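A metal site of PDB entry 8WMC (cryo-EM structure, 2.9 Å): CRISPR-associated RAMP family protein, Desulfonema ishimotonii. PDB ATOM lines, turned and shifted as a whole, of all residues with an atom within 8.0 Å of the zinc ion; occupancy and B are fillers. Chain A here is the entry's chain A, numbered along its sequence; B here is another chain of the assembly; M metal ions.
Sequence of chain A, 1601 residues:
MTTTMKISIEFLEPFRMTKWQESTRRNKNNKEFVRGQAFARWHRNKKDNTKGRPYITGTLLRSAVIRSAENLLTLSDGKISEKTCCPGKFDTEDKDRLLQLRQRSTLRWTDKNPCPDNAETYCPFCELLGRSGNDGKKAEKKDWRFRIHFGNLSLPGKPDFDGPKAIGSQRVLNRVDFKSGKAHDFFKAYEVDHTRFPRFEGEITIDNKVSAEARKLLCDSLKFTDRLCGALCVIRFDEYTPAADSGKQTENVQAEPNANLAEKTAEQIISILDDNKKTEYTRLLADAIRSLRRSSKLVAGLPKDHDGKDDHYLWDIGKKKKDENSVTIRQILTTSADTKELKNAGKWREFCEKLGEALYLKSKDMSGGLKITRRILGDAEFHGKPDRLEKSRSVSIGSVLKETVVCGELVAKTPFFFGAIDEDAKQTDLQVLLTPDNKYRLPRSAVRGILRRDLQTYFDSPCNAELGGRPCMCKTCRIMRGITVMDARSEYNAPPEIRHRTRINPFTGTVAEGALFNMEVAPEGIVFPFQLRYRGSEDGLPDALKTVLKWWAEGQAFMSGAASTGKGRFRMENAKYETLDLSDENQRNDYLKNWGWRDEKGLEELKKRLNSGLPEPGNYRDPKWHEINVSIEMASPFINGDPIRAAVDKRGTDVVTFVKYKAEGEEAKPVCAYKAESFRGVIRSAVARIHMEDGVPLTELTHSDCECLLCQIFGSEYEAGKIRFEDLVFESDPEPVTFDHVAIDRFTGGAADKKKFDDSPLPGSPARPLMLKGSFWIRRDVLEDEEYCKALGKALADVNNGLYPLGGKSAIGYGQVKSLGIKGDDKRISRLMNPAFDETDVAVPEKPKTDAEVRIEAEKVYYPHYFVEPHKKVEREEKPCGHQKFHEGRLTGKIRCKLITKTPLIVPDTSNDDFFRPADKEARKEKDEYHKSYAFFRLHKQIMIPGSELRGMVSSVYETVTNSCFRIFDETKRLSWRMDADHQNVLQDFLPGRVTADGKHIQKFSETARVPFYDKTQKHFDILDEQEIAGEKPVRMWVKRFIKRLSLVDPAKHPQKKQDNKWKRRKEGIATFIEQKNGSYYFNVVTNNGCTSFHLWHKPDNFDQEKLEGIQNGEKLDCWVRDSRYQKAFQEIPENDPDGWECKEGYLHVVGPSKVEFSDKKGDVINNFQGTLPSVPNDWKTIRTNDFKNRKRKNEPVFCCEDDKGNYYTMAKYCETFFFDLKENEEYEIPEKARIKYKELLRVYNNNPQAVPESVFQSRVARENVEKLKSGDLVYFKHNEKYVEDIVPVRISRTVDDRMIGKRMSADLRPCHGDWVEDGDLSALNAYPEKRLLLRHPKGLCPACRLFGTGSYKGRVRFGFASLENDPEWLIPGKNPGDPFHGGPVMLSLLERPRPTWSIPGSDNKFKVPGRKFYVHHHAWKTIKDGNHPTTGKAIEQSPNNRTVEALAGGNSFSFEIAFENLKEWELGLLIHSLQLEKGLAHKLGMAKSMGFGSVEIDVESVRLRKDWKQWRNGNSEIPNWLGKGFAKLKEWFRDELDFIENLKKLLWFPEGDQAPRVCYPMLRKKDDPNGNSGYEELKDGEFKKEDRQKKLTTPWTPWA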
ATOM      1  N   ARG A 452     -39.302 -24.149 -24.547  1.00  0.00           N
ATOM      2  CA  ARG A 452     -37.949 -24.555 -24.929  1.00  0.00           C
ATOM      3  C   ARG A 452     -37.614 -24.079 -26.334  1.00  0.00           C
ATOM      4  O   ARG A 452     -36.509 -23.574 -26.578  1.00  0.00           O
ATOM      5  CB  ARG A 452     -37.823 -26.081 -24.834  1.00  0.00           C
ATOM      6  CG  ARG A 452     -36.401 -26.596 -25.018  1.00  0.00           C
ATOM      7  CD  ARG A 452     -36.360 -28.115 -24.929  1.00  0.00           C
ATOM      8  NE  ARG A 452     -36.328 -28.589 -23.552  1.00  0.00           N
ATOM      9  CZ  ARG A 452     -35.238 -28.667 -22.798  1.00  0.00           C
ATOM     10  NH1 ARG A 452     -34.053 -28.300 -23.249  1.00  0.00           N
ATOM     11  NH2 ARG A 452     -35.342 -29.131 -21.552  1.00  0.00           N
ATOM     12  N   GLN A 456     -34.624 -21.420 -27.280  1.00  0.00           N
ATOM     13  CA  GLN A 456     -33.592 -21.737 -28.263  1.00  0.00           C
ATOM     14  C   GLN A 456     -33.560 -20.683 -29.362  1.00  0.00           C
ATOM     15  O   GLN A 456     -32.477 -20.289 -29.815  1.00  0.00           O
ATOM     16  CB  GLN A 456     -33.846 -23.117 -28.862  1.00  0.00           C
ATOM     17  CG  GLN A 456     -33.179 -24.246 -28.099  1.00  0.00           C
ATOM     18  CD  GLN A 456     -33.702 -25.621 -28.473  1.00  0.00           C
ATOM     19  OE1 GLN A 456     -34.795 -25.759 -29.024  1.00  0.00           O
ATOM     20  NE2 GLN A 456     -32.929 -26.651 -28.176  1.00  0.00           N
ATOM     21  N   SER A 461     -28.900 -20.782 -30.559  1.00  0.00           N
ATOM     22  CA  SER A 461     -27.949 -21.859 -30.293  1.00  0.00           C
ATOM     23  C   SER A 461     -28.741 -23.139 -30.041  1.00  0.00           C
ATOM     24  O   SER A 461     -29.215 -23.370 -28.915  1.00  0.00           O
ATOM     25  CB  SER A 461     -27.044 -21.533 -29.103  1.00  0.00           C
ATOM     26  OG  SER A 461     -26.444 -20.261 -29.255  1.00  0.00           O
ATOM     27  N   PRO A 462     -28.931 -23.993 -31.052  1.00  0.00           N
ATOM     28  CA  PRO A 462     -29.632 -25.257 -30.811  1.00  0.00           C
ATOM     29  C   PRO A 462     -28.866 -26.157 -29.851  1.00  0.00           C
ATOM     30  O   PRO A 462     -27.642 -26.146 -29.799  1.00  0.00           O
ATOM     31  CB  PRO A 462     -29.745 -25.886 -32.203  1.00  0.00           C
ATOM     32  CG  PRO A 462     -29.486 -24.790 -33.159  1.00  0.00           C
ATOM     33  CD  PRO A 462     -28.586 -23.831 -32.471  1.00  0.00           C
ATOM     34  N   CYS A 463     -29.630 -26.947 -29.091  1.00  0.00           N
ATOM     35  CA  CYS A 463     -29.074 -27.905 -28.140  1.00  0.00           C
ATOM     36  C   CYS A 463     -29.114 -29.295 -28.743  1.00  0.00           C
ATOM     37  O   CYS A 463     -30.179 -29.769 -29.147  1.00  0.00           O
ATOM     38  CB  CYS A 463     -29.862 -27.862 -26.819  1.00  0.00           C
ATOM     39  SG  CYS A 463     -29.296 -29.016 -25.555  1.00  0.00           S
ATOM     40  N   ASN A 464     -27.953 -29.960 -28.800  1.00  0.00           N
ATOM     41  CA  ASN A 464     -27.823 -31.300 -29.362  1.00  0.00           C
ATOM     42  C   ASN A 464     -27.706 -32.364 -28.283  1.00  0.00           C
ATOM     43  O   ASN A 464     -27.080 -33.407 -28.499  1.00  0.00           O
ATOM     44  CB  ASN A 464     -26.609 -31.366 -30.286  1.00  0.00           C
ATOM     45  CG  ASN A 464     -25.295 -31.280 -29.539  1.00  0.00           C
ATOM     46  OD1 ASN A 464     -25.216 -30.676 -28.482  1.00  0.00           O
ATOM     47  ND2 ASN A 464     -24.240 -31.877 -30.095  1.00  0.00           N
ATOM     48  N   ALA A 465     -28.317 -32.136 -27.127  1.00  0.00           N
ATOM     49  CA  ALA A 465     -28.241 -33.120 -26.051  1.00  0.00           C
ATOM     50  C   ALA A 465     -29.026 -34.374 -26.424  1.00  0.00           C
ATOM     51  O   ALA A 465     -29.935 -34.344 -27.259  1.00  0.00           O
ATOM     52  CB  ALA A 465     -28.770 -32.530 -24.748  1.00  0.00           C
ATOM     53  N   GLU A 466     -28.647 -35.477 -25.800  1.00  0.00           N
ATOM     54  CA  GLU A 466     -29.243 -36.790 -26.047  1.00  0.00           C
ATOM     55  C   GLU A 466     -29.727 -37.376 -24.732  1.00  0.00           C
ATOM     56  O   GLU A 466     -29.184 -37.071 -23.664  1.00  0.00           O
ATOM     57  CB  GLU A 466     -28.228 -37.730 -26.735  1.00  0.00           C
ATOM     58  CG  GLU A 466     -28.748 -39.121 -27.083  1.00  0.00           C
ATOM     59  CD  GLU A 466     -29.854 -39.098 -28.122  1.00  0.00           C
ATOM     60  OE1 GLU A 466     -29.904 -38.139 -28.923  1.00  0.00           O
ATOM     61  OE2 GLU A 466     -30.676 -40.038 -28.140  1.00  0.00           O
ATOM     62  N   PRO A 471     -26.797 -34.420 -16.658  1.00  0.00           N
ATOM     63  CA  PRO A 471     -27.606 -33.326 -17.229  1.00  0.00           C
ATOM     64  C   PRO A 471     -26.809 -32.410 -18.148  1.00  0.00           C
ATOM     65  O   PRO A 471     -25.623 -32.168 -17.937  1.00  0.00           O
ATOM     66  CB  PRO A 471     -28.098 -32.569 -15.990  1.00  0.00           C
ATOM     67  CG  PRO A 471     -27.937 -33.497 -14.865  1.00  0.00           C
ATOM     68  CD  PRO A 471     -26.755 -34.341 -15.192  1.00  0.00           C
ATOM     69  N   CYS A 472     -27.494 -31.902 -19.172  1.00  0.00           N
ATOM     70  CA  CYS A 472     -26.905 -30.900 -20.050  1.00  0.00           C
ATOM     71  C   CYS A 472     -26.678 -29.608 -19.279  1.00  0.00           C
ATOM     72  O   CYS A 472     -27.392 -29.292 -18.328  1.00  0.00           O
ATOM     73  CB  CYS A 472     -27.821 -30.653 -21.246  1.00  0.00           C
ATOM     74  SG  CYS A 472     -27.112 -29.613 -22.538  1.00  0.00           S
ATOM     75  N   MET A 473     -25.669 -28.854 -19.711  1.00  0.00           N
ATOM     76  CA  MET A 473     -25.208 -27.649 -19.012  1.00  0.00           C
ATOM     77  C   MET A 473     -25.088 -26.486 -19.980  1.00  0.00           C
ATOM     78  O   MET A 473     -24.073 -25.780 -20.025  1.00  0.00           O
ATOM     79  CB  MET A 473     -23.883 -27.940 -18.319  1.00  0.00           C
ATOM     80  CG  MET A 473     -23.491 -26.938 -17.243  1.00  0.00           C
ATOM     81  SD  MET A 473     -24.606 -26.908 -15.820  1.00  0.00           S
ATOM     82  CE  MET A 473     -24.183 -28.444 -15.019  1.00  0.00           C
ATOM     83  N   CYS A 474     -26.132 -26.267 -20.767  1.00  0.00           N
ATOM     84  CA  CYS A 474     -26.254 -25.110 -21.653  1.00  0.00           C
ATOM     85  C   CYS A 474     -27.286 -24.146 -21.083  1.00  0.00           C
ATOM     86  O   CYS A 474     -27.977 -24.448 -20.099  1.00  0.00           O
ATOM     87  CB  CYS A 474     -26.650 -25.551 -23.071  1.00  0.00           C
ATOM     88  SG  CYS A 474     -28.363 -26.097 -23.252  1.00  0.00           S
ATOM     89  N   LYS A 475     -27.370 -22.971 -21.700  1.00  0.00           N
ATOM     90  CA  LYS A 475     -28.210 -21.903 -21.152  1.00  0.00           C
ATOM     91  C   LYS A 475     -29.685 -22.305 -21.141  1.00  0.00           C
ATOM     92  O   LYS A 475     -30.389 -22.100 -20.141  1.00  0.00           O
ATOM     93  CB  LYS A 475     -28.016 -20.623 -21.973  1.00  0.00           C
ATOM     94  CG  LYS A 475     -26.598 -20.066 -21.956  1.00  0.00           C
ATOM     95  CD  LYS A 475     -26.409 -19.046 -23.059  1.00  0.00           C
ATOM     96  CE  LYS A 475     -25.021 -18.425 -23.012  1.00  0.00           C
ATOM     97  NZ  LYS A 475     -24.749 -17.576 -24.208  1.00  0.00           N
ATOM     98  N   THR A 476     -30.164 -22.888 -22.235  1.00  0.00           N
ATOM     99  CA  THR A 476     -31.576 -23.246 -22.321  1.00  0.00           C
ATOM    100  C   THR A 476     -31.939 -24.319 -21.301  1.00  0.00           C
ATOM    101  O   THR A 476     -32.958 -24.206 -20.614  1.00  0.00           O
ATOM    102  CB  THR A 476     -31.913 -23.727 -23.737  1.00  0.00           C
ATOM    103  OG1 THR A 476     -31.411 -22.784 -24.693  1.00  0.00           O
ATOM    104  CG2 THR A 476     -33.406 -23.876 -23.913  1.00  0.00           C
ATOM    105  N   CYS A 477     -31.122 -25.367 -21.199  1.00  0.00           N
ATOM    106  CA  CYS A 477     -31.405 -26.431 -20.256  1.00  0.00           C
ATOM    107  C   CYS A 477     -31.324 -25.925 -18.815  1.00  0.00           C
ATOM    108  O   CYS A 477     -32.156 -26.287 -17.970  1.00  0.00           O
ATOM    109  CB  CYS A 477     -30.438 -27.592 -20.470  1.00  0.00           C
ATOM    110  SG  CYS A 477     -30.780 -28.579 -21.959  1.00  0.00           S
ATOM    111  N   ARG A 478     -30.329 -25.076 -18.518  1.00  0.00           N
ATOM    112  CA  ARG A 478     -30.202 -24.516 -17.185  1.00  0.00           C
ATOM    113  C   ARG A 478     -31.423 -23.683 -16.814  1.00  0.00           C
ATOM    114  O   ARG A 478     -31.919 -23.771 -15.687  1.00  0.00           O
ATOM    115  CB  ARG A 478     -28.936 -23.676 -17.084  1.00  0.00           C
ATOM    116  CG  ARG A 478     -27.678 -24.475 -16.764  1.00  0.00           C
ATOM    117  CD  ARG A 478     -26.521 -23.576 -16.325  1.00  0.00           C
ATOM    118  NE  ARG A 478     -25.804 -23.035 -17.472  1.00  0.00           N
ATOM    119  CZ  ARG A 478     -25.447 -21.765 -17.663  1.00  0.00           C
ATOM    120  NH1 ARG A 478     -25.711 -20.815 -16.771  1.00  0.00           N
ATOM    121  NH2 ARG A 478     -24.801 -21.429 -18.774  1.00  0.00           N
ATOM    122  N   ARG A 481     -34.551 -26.036 -16.295  1.00  0.00           N
ATOM    123  CA  ARG A 481     -34.560 -26.945 -15.154  1.00  0.00           C
ATOM    124  C   ARG A 481     -35.300 -26.365 -13.945  1.00  0.00           C
ATOM    125  O   ARG A 481     -35.733 -27.141 -13.092  1.00  0.00           O
ATOM    126  CB  ARG A 481     -33.128 -27.316 -14.739  1.00  0.00           C
ATOM    127  CG  ARG A 481     -32.736 -28.755 -15.066  1.00  0.00           C
ATOM    128  CD  ARG A 481     -31.509 -29.201 -14.281  1.00  0.00           C
ATOM    129  NE  ARG A 481     -30.285 -28.579 -14.771  1.00  0.00           N
ATOM    130  CZ  ARG A 481     -29.659 -28.904 -15.898  1.00  0.00           C
ATOM    131  NH1 ARG A 481     -30.122 -29.841 -16.709  1.00  0.00           N
ATOM    132  NH2 ARG A 481     -28.546 -28.259 -16.223  1.00  0.00           N
ATOM    133  N   MET B 620     -22.482 -25.648 -30.668  1.00  0.00           N
ATOM    134  CA  MET B 620     -22.182 -27.021 -30.288  1.00  0.00           C
ATOM    135  C   MET B 620     -22.361 -27.985 -31.452  1.00  0.00           C
ATOM    136  O   MET B 620     -21.690 -29.026 -31.518  1.00  0.00           O
ATOM    137  CB  MET B 620     -23.053 -27.434 -29.096  1.00  0.00           C
ATOM    138  CG  MET B 620     -23.041 -26.394 -27.939  1.00  0.00           C
ATOM    139  SD  MET B 620     -24.002 -26.740 -26.445  1.00  0.00           S
ATOM    140  CE  MET B 620     -25.421 -27.632 -27.072  1.00  0.00           C
HETATM  141 ZN    ZN M   1     -28.910 -28.359 -23.347  1.00  0.00          ZN
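NH2 of Arg 481 sits at hydrogen-bond distance from O of Cys 472 (2.6 Å).
The backbone NH of Cys 463 sits close to the side-chain amide nitrogen of Gln 456 (3.4 Å).
N of Ala 465 sits close to SG of Cys 463, 3.6 Å away.
SG of Cys 477 sits close to NH1 of Arg 452, at 3.5 Å.
The zinc ion is bound by the side-chain sulfur (SG) of Cys 474 (2.3 Å), the side-chain sulfur (SG) of Cys 463 (2.3 Å), the side-chain sulfur (SG) of Cys 472 (2.3 Å) and the side-chain sulfur (SG) of Cys 477 (2.3 Å).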
